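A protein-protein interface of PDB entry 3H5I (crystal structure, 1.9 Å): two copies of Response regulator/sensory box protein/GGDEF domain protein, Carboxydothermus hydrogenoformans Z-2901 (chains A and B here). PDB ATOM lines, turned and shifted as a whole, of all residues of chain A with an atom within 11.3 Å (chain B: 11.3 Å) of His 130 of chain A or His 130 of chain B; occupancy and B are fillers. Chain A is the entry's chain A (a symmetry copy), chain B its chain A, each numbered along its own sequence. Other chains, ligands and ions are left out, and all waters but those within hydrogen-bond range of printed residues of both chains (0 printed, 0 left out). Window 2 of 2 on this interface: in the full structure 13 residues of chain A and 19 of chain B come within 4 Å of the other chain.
CD of Arg 123 of chain A touches CE2 of Tyr 102 of chain B, 3.7 Å away.
CD2 of Leu 124 of chain A touches CD2 of Leu 124 of chain B, 3.2 Å away.
Glu 126 of chain A touches Asn 128 of chain B (OE1 to OD1, 3.8 Å).
CB of Ala 127 of chain B touches CB of Ala 127 of chain A, at 3.7 Å.
His 130 of chain B touches His 130 of chain A (CD2 to NE2, 3.6 Å).
O of Leu 124 of chain B lies within hydrogen-bond range of ND2 of Asn 128 of chain B (3.0 Å).
The backbone carbonyl oxygen of Leu 124 of chain A lies within hydrogen-bond range of the side-chain amide nitrogen of Asn 128 of chain A, at 3.0 Å.
Arg 123 of chain A touches Tyr 102 of chain B, but with the chains exchanged Tyr 102 of chain A does not touch Arg 123 of chain B (12.6 Å).
Glu 126 of chain A touches Asn 128 of chain B, but with the chains exchanged Asn 128 of chain A does not touch Glu 126 of chain B (10.1 Å).
Ala 127 of chain A touches its own counterpart, Ala 127 of chain B.
His 130 of chain B touches its own counterpart, His 130 of chain A.
Of the 6 pairs that touch across the chains among the printed residues, 3 have their exchanged pair printed and touching as well.
Hydrophobic or aromatic side chains of chain A that line the printed part of chain B: Leu 124, Ala 127 and His 130.
Hydrophobic or aromatic side chains of chain B that line the printed part of chain A: Tyr 102, Leu 124, Ala 127 and His 130.
Among the printed residues, 6 pairs touch across the chains.
OD1 of Asn 128 of chain B sits close to O of Arg 123 of chain A.
His 130 of chain A touches one residue of chain B.
Of chain A, only His 130 comes within 4 Å of His 130 of chain B.
Of chain B, only Ala 127 comes within 4 Å of Ala 127 of chain A.
No residue of chain B comes within 4 Å of Val 129 of chain A.
Ala 127 of chain B touches one residue of chain A.
No residue of chain A comes within 4 Å of Val 129 of chain B.
Of the printed residues of chain A, Leu 124 of chain B touches Leu 124 (3.2 Å).
Printed residues of chain A within 4 Å of Asn 128 of chain B: Arg 123 and Glu 126.
Of the printed residues of chain B, Arg 123 of chain A touches Tyr 102 (3.7 Å) and Asn 128 (3.4 Å).
Of the printed residues of chain A, Tyr 102 of chain B touches Arg 123.
The nearest residue of chain A that does not touch His 130 of chain B is Ala 127 of chain A (6.9 Å).
The nearest printed residue of chain B that does not touch Glu 126 of chain A is Ala 127 of chain B (6.2 Å).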
ATOM      1  N   GLU A  78       0.214  33.293  19.717  1.00  0.00           N
ATOM      2  CA  GLU A  78       1.194  32.228  19.828  1.00  0.00           C
ATOM      3  C   GLU A  78       1.272  31.854  21.340  1.00  0.00           C
ATOM      4  O   GLU A  78       1.899  32.550  22.170  1.00  0.00           O
ATOM      5  CB  GLU A  78       2.566  32.682  19.252  1.00  0.00           C
ATOM      6  N   PRO A  80       1.805  28.299  23.808  1.00  0.00           N
ATOM      7  CA  PRO A  80       2.190  26.887  23.714  1.00  0.00           C
ATOM      8  C   PRO A  80       1.014  25.933  23.969  1.00  0.00           C
ATOM      9  O   PRO A  80       0.284  26.091  24.957  1.00  0.00           O
ATOM     10  CB  PRO A  80       3.240  26.710  24.799  1.00  0.00           C
ATOM     11  CG  PRO A  80       3.128  27.905  25.679  1.00  0.00           C
ATOM     12  CD  PRO A  80       2.287  28.941  25.025  1.00  0.00           C
ATOM     13  N   TYR A 102       4.061  21.717  21.497  1.00  0.00           N
ATOM     14  CA  TYR A 102       5.202  21.637  22.391  1.00  0.00           C
ATOM     15  C   TYR A 102       5.352  20.250  23.016  1.00  0.00           C
ATOM     16  O   TYR A 102       6.348  19.977  23.681  1.00  0.00           O
ATOM     17  CB  TYR A 102       5.106  22.662  23.506  1.00  0.00           C
ATOM     18  CG  TYR A 102       5.535  24.045  23.079  1.00  0.00           C
ATOM     19  CD1 TYR A 102       4.813  24.751  22.107  1.00  0.00           C
ATOM     20  CD2 TYR A 102       6.685  24.621  23.607  1.00  0.00           C
ATOM     21  CE1 TYR A 102       5.214  26.018  21.692  1.00  0.00           C
ATOM     22  CE2 TYR A 102       7.091  25.888  23.202  1.00  0.00           C
ATOM     23  CZ  TYR A 102       6.353  26.580  22.253  1.00  0.00           C
ATOM     24  OH  TYR A 102       6.778  27.836  21.878  1.00  0.00           O
ATOM     25  N   ALA A 121       7.713  23.086  28.560  1.00  0.00           N
ATOM     26  CA  ALA A 121       6.979  23.889  27.560  1.00  0.00           C
ATOM     27  C   ALA A 121       6.944  25.385  27.940  1.00  0.00           C
ATOM     28  O   ALA A 121       7.139  26.263  27.092  1.00  0.00           O
ATOM     29  CB  ALA A 121       5.531  23.352  27.401  1.00  0.00           C
ATOM     30  N   LEU A 122       6.728  25.649  29.221  1.00  0.00           N
ATOM     31  CA  LEU A 122       6.692  27.006  29.753  1.00  0.00           C
ATOM     32  C   LEU A 122       8.057  27.715  29.491  1.00  0.00           C
ATOM     33  O   LEU A 122       8.079  28.832  28.974  1.00  0.00           O
ATOM     34  CB  LEU A 122       6.302  26.993  31.235  1.00  0.00           C
ATOM     35  CG  LEU A 122       4.801  26.716  31.515  1.00  0.00           C
ATOM     36  CD1 LEU A 122       4.517  26.482  32.981  1.00  0.00           C
ATOM     37  CD2 LEU A 122       3.882  27.827  30.941  1.00  0.00           C
ATOM     38  N   ARG A 123       9.161  27.033  29.774  1.00  0.00           N
ATOM     39  CA  ARG A 123      10.502  27.602  29.517  1.00  0.00           C
ATOM     40  C   ARG A 123      10.865  27.682  28.030  1.00  0.00           C
ATOM     41  O   ARG A 123      11.432  28.691  27.589  1.00  0.00           O
ATOM     42  CB  ARG A 123      11.592  26.847  30.264  1.00  0.00           C
ATOM     43  CG  ARG A 123      11.203  26.262  31.573  1.00  0.00           C
ATOM     44  CD  ARG A 123      12.205  26.488  32.695  1.00  0.00           C
ATOM     45  NE  ARG A 123      11.614  26.063  33.955  1.00  0.00           N
ATOM     46  CZ  ARG A 123      10.542  26.633  34.529  1.00  0.00           C
ATOM     47  NH1 ARG A 123       9.928  27.687  33.989  1.00  0.00           N
ATOM     48  NH2 ARG A 123      10.061  26.149  35.672  1.00  0.00           N
ATOM     49  N   LEU A 124      10.557  26.639  27.254  1.00  0.00           N
ATOM     50  CA  LEU A 124      10.782  26.669  25.803  1.00  0.00           C
ATOM     51  C   LEU A 124       9.998  27.811  25.145  1.00  0.00           C
ATOM     52  O   LEU A 124      10.441  28.370  24.137  1.00  0.00           O
ATOM     53  CB  LEU A 124      10.395  25.345  25.126  1.00  0.00           C
ATOM     54  CG  LEU A 124      11.282  24.119  25.339  1.00  0.00           C
ATOM     55  CD1 LEU A 124      10.619  22.791  24.871  1.00  0.00           C
ATOM     56  CD2 LEU A 124      12.592  24.358  24.627  1.00  0.00           C
ATOM     57  N   TYR A 125       8.837  28.149  25.703  1.00  0.00           N
ATOM     58  CA  TYR A 125       7.993  29.191  25.121  1.00  0.00           C
ATOM     59  C   TYR A 125       8.676  30.553  25.262  1.00  0.00           C
ATOM     60  O   TYR A 125       8.833  31.275  24.258  1.00  0.00           O
ATOM     61  CB  TYR A 125       6.608  29.200  25.769  1.00  0.00           C
ATOM     62  CG  TYR A 125       5.726  30.365  25.360  1.00  0.00           C
ATOM     63  CD1 TYR A 125       5.533  30.690  24.013  1.00  0.00           C
ATOM     64  CD2 TYR A 125       5.058  31.126  26.328  1.00  0.00           C
ATOM     65  CE1 TYR A 125       4.719  31.761  23.640  1.00  0.00           C
ATOM     66  CE2 TYR A 125       4.239  32.195  25.965  1.00  0.00           C
ATOM     67  CZ  TYR A 125       4.082  32.506  24.623  1.00  0.00           C
ATOM     68  OH  TYR A 125       3.267  33.552  24.276  1.00  0.00           O
ATOM     69  N   GLU A 126       9.082  30.877  26.488  1.00  0.00           N
ATOM     70  CA  GLU A 126       9.881  32.083  26.780  1.00  0.00           C
ATOM     71  C   GLU A 126      11.156  32.212  25.912  1.00  0.00           C
ATOM     72  O   GLU A 126      11.463  33.289  25.399  1.00  0.00           O
ATOM     73  CB  GLU A 126      10.285  32.097  28.259  1.00  0.00           C
ATOM     74  CG  GLU A 126       9.103  32.213  29.225  1.00  0.00           C
ATOM     75  CD  GLU A 126       9.398  31.626  30.603  1.00  0.00           C
ATOM     76  OE1 GLU A 126      10.582  31.657  31.027  1.00  0.00           O
ATOM     77  OE2 GLU A 126       8.441  31.132  31.257  1.00  0.00           O
ATOM     78  N   ALA A 127      11.889  31.108  25.761  1.00  0.00           N
ATOM     79  CA  ALA A 127      13.084  31.057  24.901  1.00  0.00           C
ATOM     80  C   ALA A 127      12.812  31.425  23.427  1.00  0.00           C
ATOM     81  O   ALA A 127      13.593  32.173  22.825  1.00  0.00           O
ATOM     82  CB  ALA A 127      13.729  29.674  24.981  1.00  0.00           C
ATOM     83  N   ASN A 128      11.724  30.896  22.850  1.00  0.00           N
ATOM     84  CA  ASN A 128      11.331  31.223  21.463  1.00  0.00           C
ATOM     85  C   ASN A 128      10.617  32.588  21.374  1.00  0.00           C
ATOM     86  O   ASN A 128      10.874  33.359  20.445  1.00  0.00           O
ATOM     87  CB  ASN A 128      10.423  30.137  20.839  1.00  0.00           C
ATOM     88  CG  ASN A 128      11.064  28.729  20.817  1.00  0.00           C
ATOM     89  OD1 ASN A 128      12.234  28.548  20.451  1.00  0.00           O
ATOM     90  ND2 ASN A 128      10.270  27.726  21.192  1.00  0.00           N
ATOM     91  N   VAL A 129       9.719  32.873  22.327  1.00  0.00           N
ATOM     92  CA  VAL A 129       8.930  34.130  22.337  1.00  0.00           C
ATOM     93  C   VAL A 129       9.826  35.355  22.554  1.00  0.00           C
ATOM     94  O   VAL A 129       9.486  36.464  22.125  1.00  0.00           O
ATOM     95  CB  VAL A 129       7.799  34.126  23.411  1.00  0.00           C
ATOM     96  N   HIS A 130      10.954  35.144  23.231  1.00  0.00           N
ATOM     97  CA  HIS A 130      12.081  36.087  23.231  1.00  0.00           C
ATOM     98  C   HIS A 130      12.278  36.856  21.895  1.00  0.00           C
ATOM     99  O   HIS A 130      13.011  36.430  20.993  1.00  0.00           O
ATOM    100  CB  HIS A 130      13.354  35.314  23.588  1.00  0.00           C
ATOM    101  CG  HIS A 130      14.565  36.170  23.747  1.00  0.00           C
ATOM    102  ND1 HIS A 130      14.676  37.135  24.727  1.00  0.00           N
ATOM    103  CD2 HIS A 130      15.732  36.189  23.063  1.00  0.00           C
ATOM    104  CE1 HIS A 130      15.855  37.724  24.631  1.00  0.00           C
ATOM    105  NE2 HIS A 130      16.516  37.167  23.629  1.00  0.00           N
ATOM    106  N   GLU B  78      20.458  31.416  40.563  1.00  0.00           N
ATOM    107  CA  GLU B  78      19.507  30.781  39.668  1.00  0.00           C
ATOM    108  C   GLU B  78      20.266  29.605  38.980  1.00  0.00           C
ATOM    109  O   GLU B  78      21.068  29.788  38.037  1.00  0.00           O
ATOM    110  CB  GLU B  78      18.943  31.809  38.646  1.00  0.00           C
ATOM    111  N   PRO B  80      19.455  25.549  37.602  1.00  0.00           N
ATOM    112  CA  PRO B  80      18.344  24.627  37.348  1.00  0.00           C
ATOM    113  C   PRO B  80      18.300  23.460  38.346  1.00  0.00           C
ATOM    114  O   PRO B  80      19.323  22.806  38.587  1.00  0.00           O
ATOM    115  CB  PRO B  80      18.609  24.096  35.948  1.00  0.00           C
ATOM    116  CG  PRO B  80      20.020  24.447  35.634  1.00  0.00           C
ATOM    117  CD  PRO B  80      20.534  25.422  36.631  1.00  0.00           C
ATOM    118  N   TYR B 102      12.842  22.491  36.779  1.00  0.00           N
ATOM    119  CA  TYR B 102      13.009  22.171  35.372  1.00  0.00           C
ATOM    120  C   TYR B 102      12.482  20.778  35.030  1.00  0.00           C
ATOM    121  O   TYR B 102      12.418  20.415  33.859  1.00  0.00           O
ATOM    122  CB  TYR B 102      14.465  22.255  34.954  1.00  0.00           C
ATOM    123  CG  TYR B 102      14.925  23.669  34.690  1.00  0.00           C
ATOM    124  CD1 TYR B 102      14.969  24.614  35.724  1.00  0.00           C
ATOM    125  CD2 TYR B 102      15.266  24.070  33.403  1.00  0.00           C
ATOM    126  CE1 TYR B 102      15.372  25.924  35.484  1.00  0.00           C
ATOM    127  CE2 TYR B 102      15.675  25.376  33.154  1.00  0.00           C
ATOM    128  CZ  TYR B 102      15.730  26.293  34.193  1.00  0.00           C
ATOM    129  OH  TYR B 102      16.145  27.576  33.916  1.00  0.00           O
ATOM    130  N   ALA B 121      17.286  20.173  30.457  1.00  0.00           N
ATOM    131  CA  ALA B 121      17.378  21.205  31.511  1.00  0.00           C
ATOM    132  C   ALA B 121      18.619  22.105  31.325  1.00  0.00           C
ATOM    133  O   ALA B 121      18.547  23.330  31.467  1.00  0.00           O
ATOM    134  CB  ALA B 121      17.415  20.538  32.912  1.00  0.00           C
ATOM    135  N   LEU B 122      19.736  21.481  30.974  1.00  0.00           N
ATOM    136  CA  LEU B 122      20.990  22.183  30.731  1.00  0.00           C
ATOM    137  C   LEU B 122      20.806  23.214  29.574  1.00  0.00           C
ATOM    138  O   LEU B 122      21.171  24.379  29.727  1.00  0.00           O
ATOM    139  CB  LEU B 122      22.123  21.185  30.465  1.00  0.00           C
ATOM    140  CG  LEU B 122      22.646  20.438  31.721  1.00  0.00           C
ATOM    141  CD1 LEU B 122      23.587  19.308  31.374  1.00  0.00           C
ATOM    142  CD2 LEU B 122      23.290  21.403  32.753  1.00  0.00           C
ATOM    143  N   ARG B 123      20.179  22.796  28.481  1.00  0.00           N
ATOM    144  CA  ARG B 123      19.916  23.711  27.349  1.00  0.00           C
ATOM    145  C   ARG B 123      18.833  24.756  27.639  1.00  0.00           C
ATOM    146  O   ARG B 123      18.994  25.927  27.270  1.00  0.00           O
ATOM    147  CB  ARG B 123      19.560  22.955  26.077  1.00  0.00           C
ATOM    148  CG  ARG B 123      20.204  21.626  25.905  1.00  0.00           C
ATOM    149  CD  ARG B 123      20.772  21.368  24.518  1.00  0.00           C
ATOM    150  NE  ARG B 123      21.554  20.142  24.543  1.00  0.00           N
ATOM    151  CZ  ARG B 123      22.681  19.966  25.254  1.00  0.00           C
ATOM    152  NH1 ARG B 123      23.207  20.942  25.996  1.00  0.00           N
ATOM    153  NH2 ARG B 123      23.308  18.792  25.231  1.00  0.00           N
ATOM    154  N   LEU B 124      17.733  24.355  28.284  1.00  0.00           N
ATOM    155  CA  LEU B 124      16.688  25.307  28.686  1.00  0.00           C
ATOM    156  C   LEU B 124      17.250  26.379  29.627  1.00  0.00           C
ATOM    157  O   LEU B 124      16.777  27.520  29.626  1.00  0.00           O
ATOM    158  CB  LEU B 124      15.501  24.614  29.372  1.00  0.00           C
ATOM    159  CG  LEU B 124      14.548  23.771  28.526  1.00  0.00           C
ATOM    160  CD1 LEU B 124      13.595  22.882  29.375  1.00  0.00           C
ATOM    161  CD2 LEU B 124      13.772  24.703  27.625  1.00  0.00           C
ATOM    162  N   TYR B 125      18.245  26.015  30.435  1.00  0.00           N
ATOM    163  CA  TYR B 125      18.814  26.951  31.403  1.00  0.00           C
ATOM    164  C   TYR B 125      19.560  28.069  30.672  1.00  0.00           C
ATOM    165  O   TYR B 125      19.293  29.260  30.920  1.00  0.00           O
ATOM    166  CB  TYR B 125      19.734  26.229  32.388  1.00  0.00           C
ATOM    167  CG  TYR B 125      20.513  27.144  33.315  1.00  0.00           C
ATOM    168  CD1 TYR B 125      19.874  28.155  34.041  1.00  0.00           C
ATOM    169  CD2 TYR B 125      21.892  26.976  33.486  1.00  0.00           C
ATOM    170  CE1 TYR B 125      20.592  28.994  34.893  1.00  0.00           C
ATOM    171  CE2 TYR B 125      22.619  27.806  34.339  1.00  0.00           C
ATOM    172  CZ  TYR B 125      21.962  28.812  35.031  1.00  0.00           C
ATOM    173  OH  TYR B 125      22.683  29.616  35.874  1.00  0.00           O
ATOM    174  N   GLU B 126      20.465  27.676  29.778  1.00  0.00           N
ATOM    175  CA  GLU B 126      21.174  28.612  28.882  1.00  0.00           C
ATOM    176  C   GLU B 126      20.232  29.545  28.083  1.00  0.00           C
ATOM    177  O   GLU B 126      20.478  30.748  27.979  1.00  0.00           O
ATOM    178  CB  GLU B 126      22.050  27.831  27.897  1.00  0.00           C
ATOM    179  CG  GLU B 126      23.187  27.048  28.561  1.00  0.00           C
ATOM    180  CD  GLU B 126      23.642  25.844  27.740  1.00  0.00           C
ATOM    181  OE1 GLU B 126      23.546  25.902  26.486  1.00  0.00           O
ATOM    182  OE2 GLU B 126      24.092  24.841  28.354  1.00  0.00           O
ATOM    183  N   ALA B 127      19.163  28.977  27.525  1.00  0.00           N
ATOM    184  CA  ALA B 127      18.136  29.748  26.803  1.00  0.00           C
ATOM    185  C   ALA B 127      17.466  30.849  27.652  1.00  0.00           C
ATOM    186  O   ALA B 127      17.276  31.971  27.166  1.00  0.00           O
ATOM    187  CB  ALA B 127      17.074  28.807  26.238  1.00  0.00           C
ATOM    188  N   ASN B 128      17.103  30.528  28.901  1.00  0.00           N
ATOM    189  CA  ASN B 128      16.506  31.516  29.825  1.00  0.00           C
ATOM    190  C   ASN B 128      17.575  32.431  30.457  1.00  0.00           C
ATOM    191  O   ASN B 128      17.355  33.640  30.582  1.00  0.00           O
ATOM    192  CB  ASN B 128      15.687  30.843  30.954  1.00  0.00           C
ATOM    193  CG  ASN B 128      14.540  29.944  30.435  1.00  0.00           C
ATOM    194  OD1 ASN B 128      13.773  30.314  29.534  1.00  0.00           O
ATOM    195  ND2 ASN B 128      14.414  28.762  31.038  1.00  0.00           N
ATOM    196  N   VAL B 129      18.715  31.854  30.862  1.00  0.00           N
ATOM    197  CA  VAL B 129      19.806  32.610  31.524  1.00  0.00           C
ATOM    198  C   VAL B 129      20.443  33.630  30.573  1.00  0.00           C
ATOM    199  O   VAL B 129      20.987  34.647  31.017  1.00  0.00           O
ATOM    200  CB  VAL B 129      20.920  31.683  32.102  1.00  0.00           C
ATOM    201  N   HIS B 130      20.380  33.338  29.274  1.00  0.00           N
ATOM    202  CA  HIS B 130      20.608  34.331  28.215  1.00  0.00           C
ATOM    203  C   HIS B 130      20.132  35.768  28.565  1.00  0.00           C
ATOM    204  O   HIS B 130      18.992  36.166  28.294  1.00  0.00           O
ATOM    205  CB  HIS B 130      19.915  33.840  26.940  1.00  0.00           C
ATOM    206  CG  HIS B 130      20.165  34.691  25.741  1.00  0.00           C
ATOM    207  ND1 HIS B 130      21.419  34.862  25.194  1.00  0.00           N
ATOM    208  CD2 HIS B 130      19.314  35.403  24.968  1.00  0.00           C
ATOM    209  CE1 HIS B 130      21.333  35.655  24.141  1.00  0.00           C
ATOM    210  NE2 HIS B 130      20.065  35.998  23.982  1.00  0.00           N
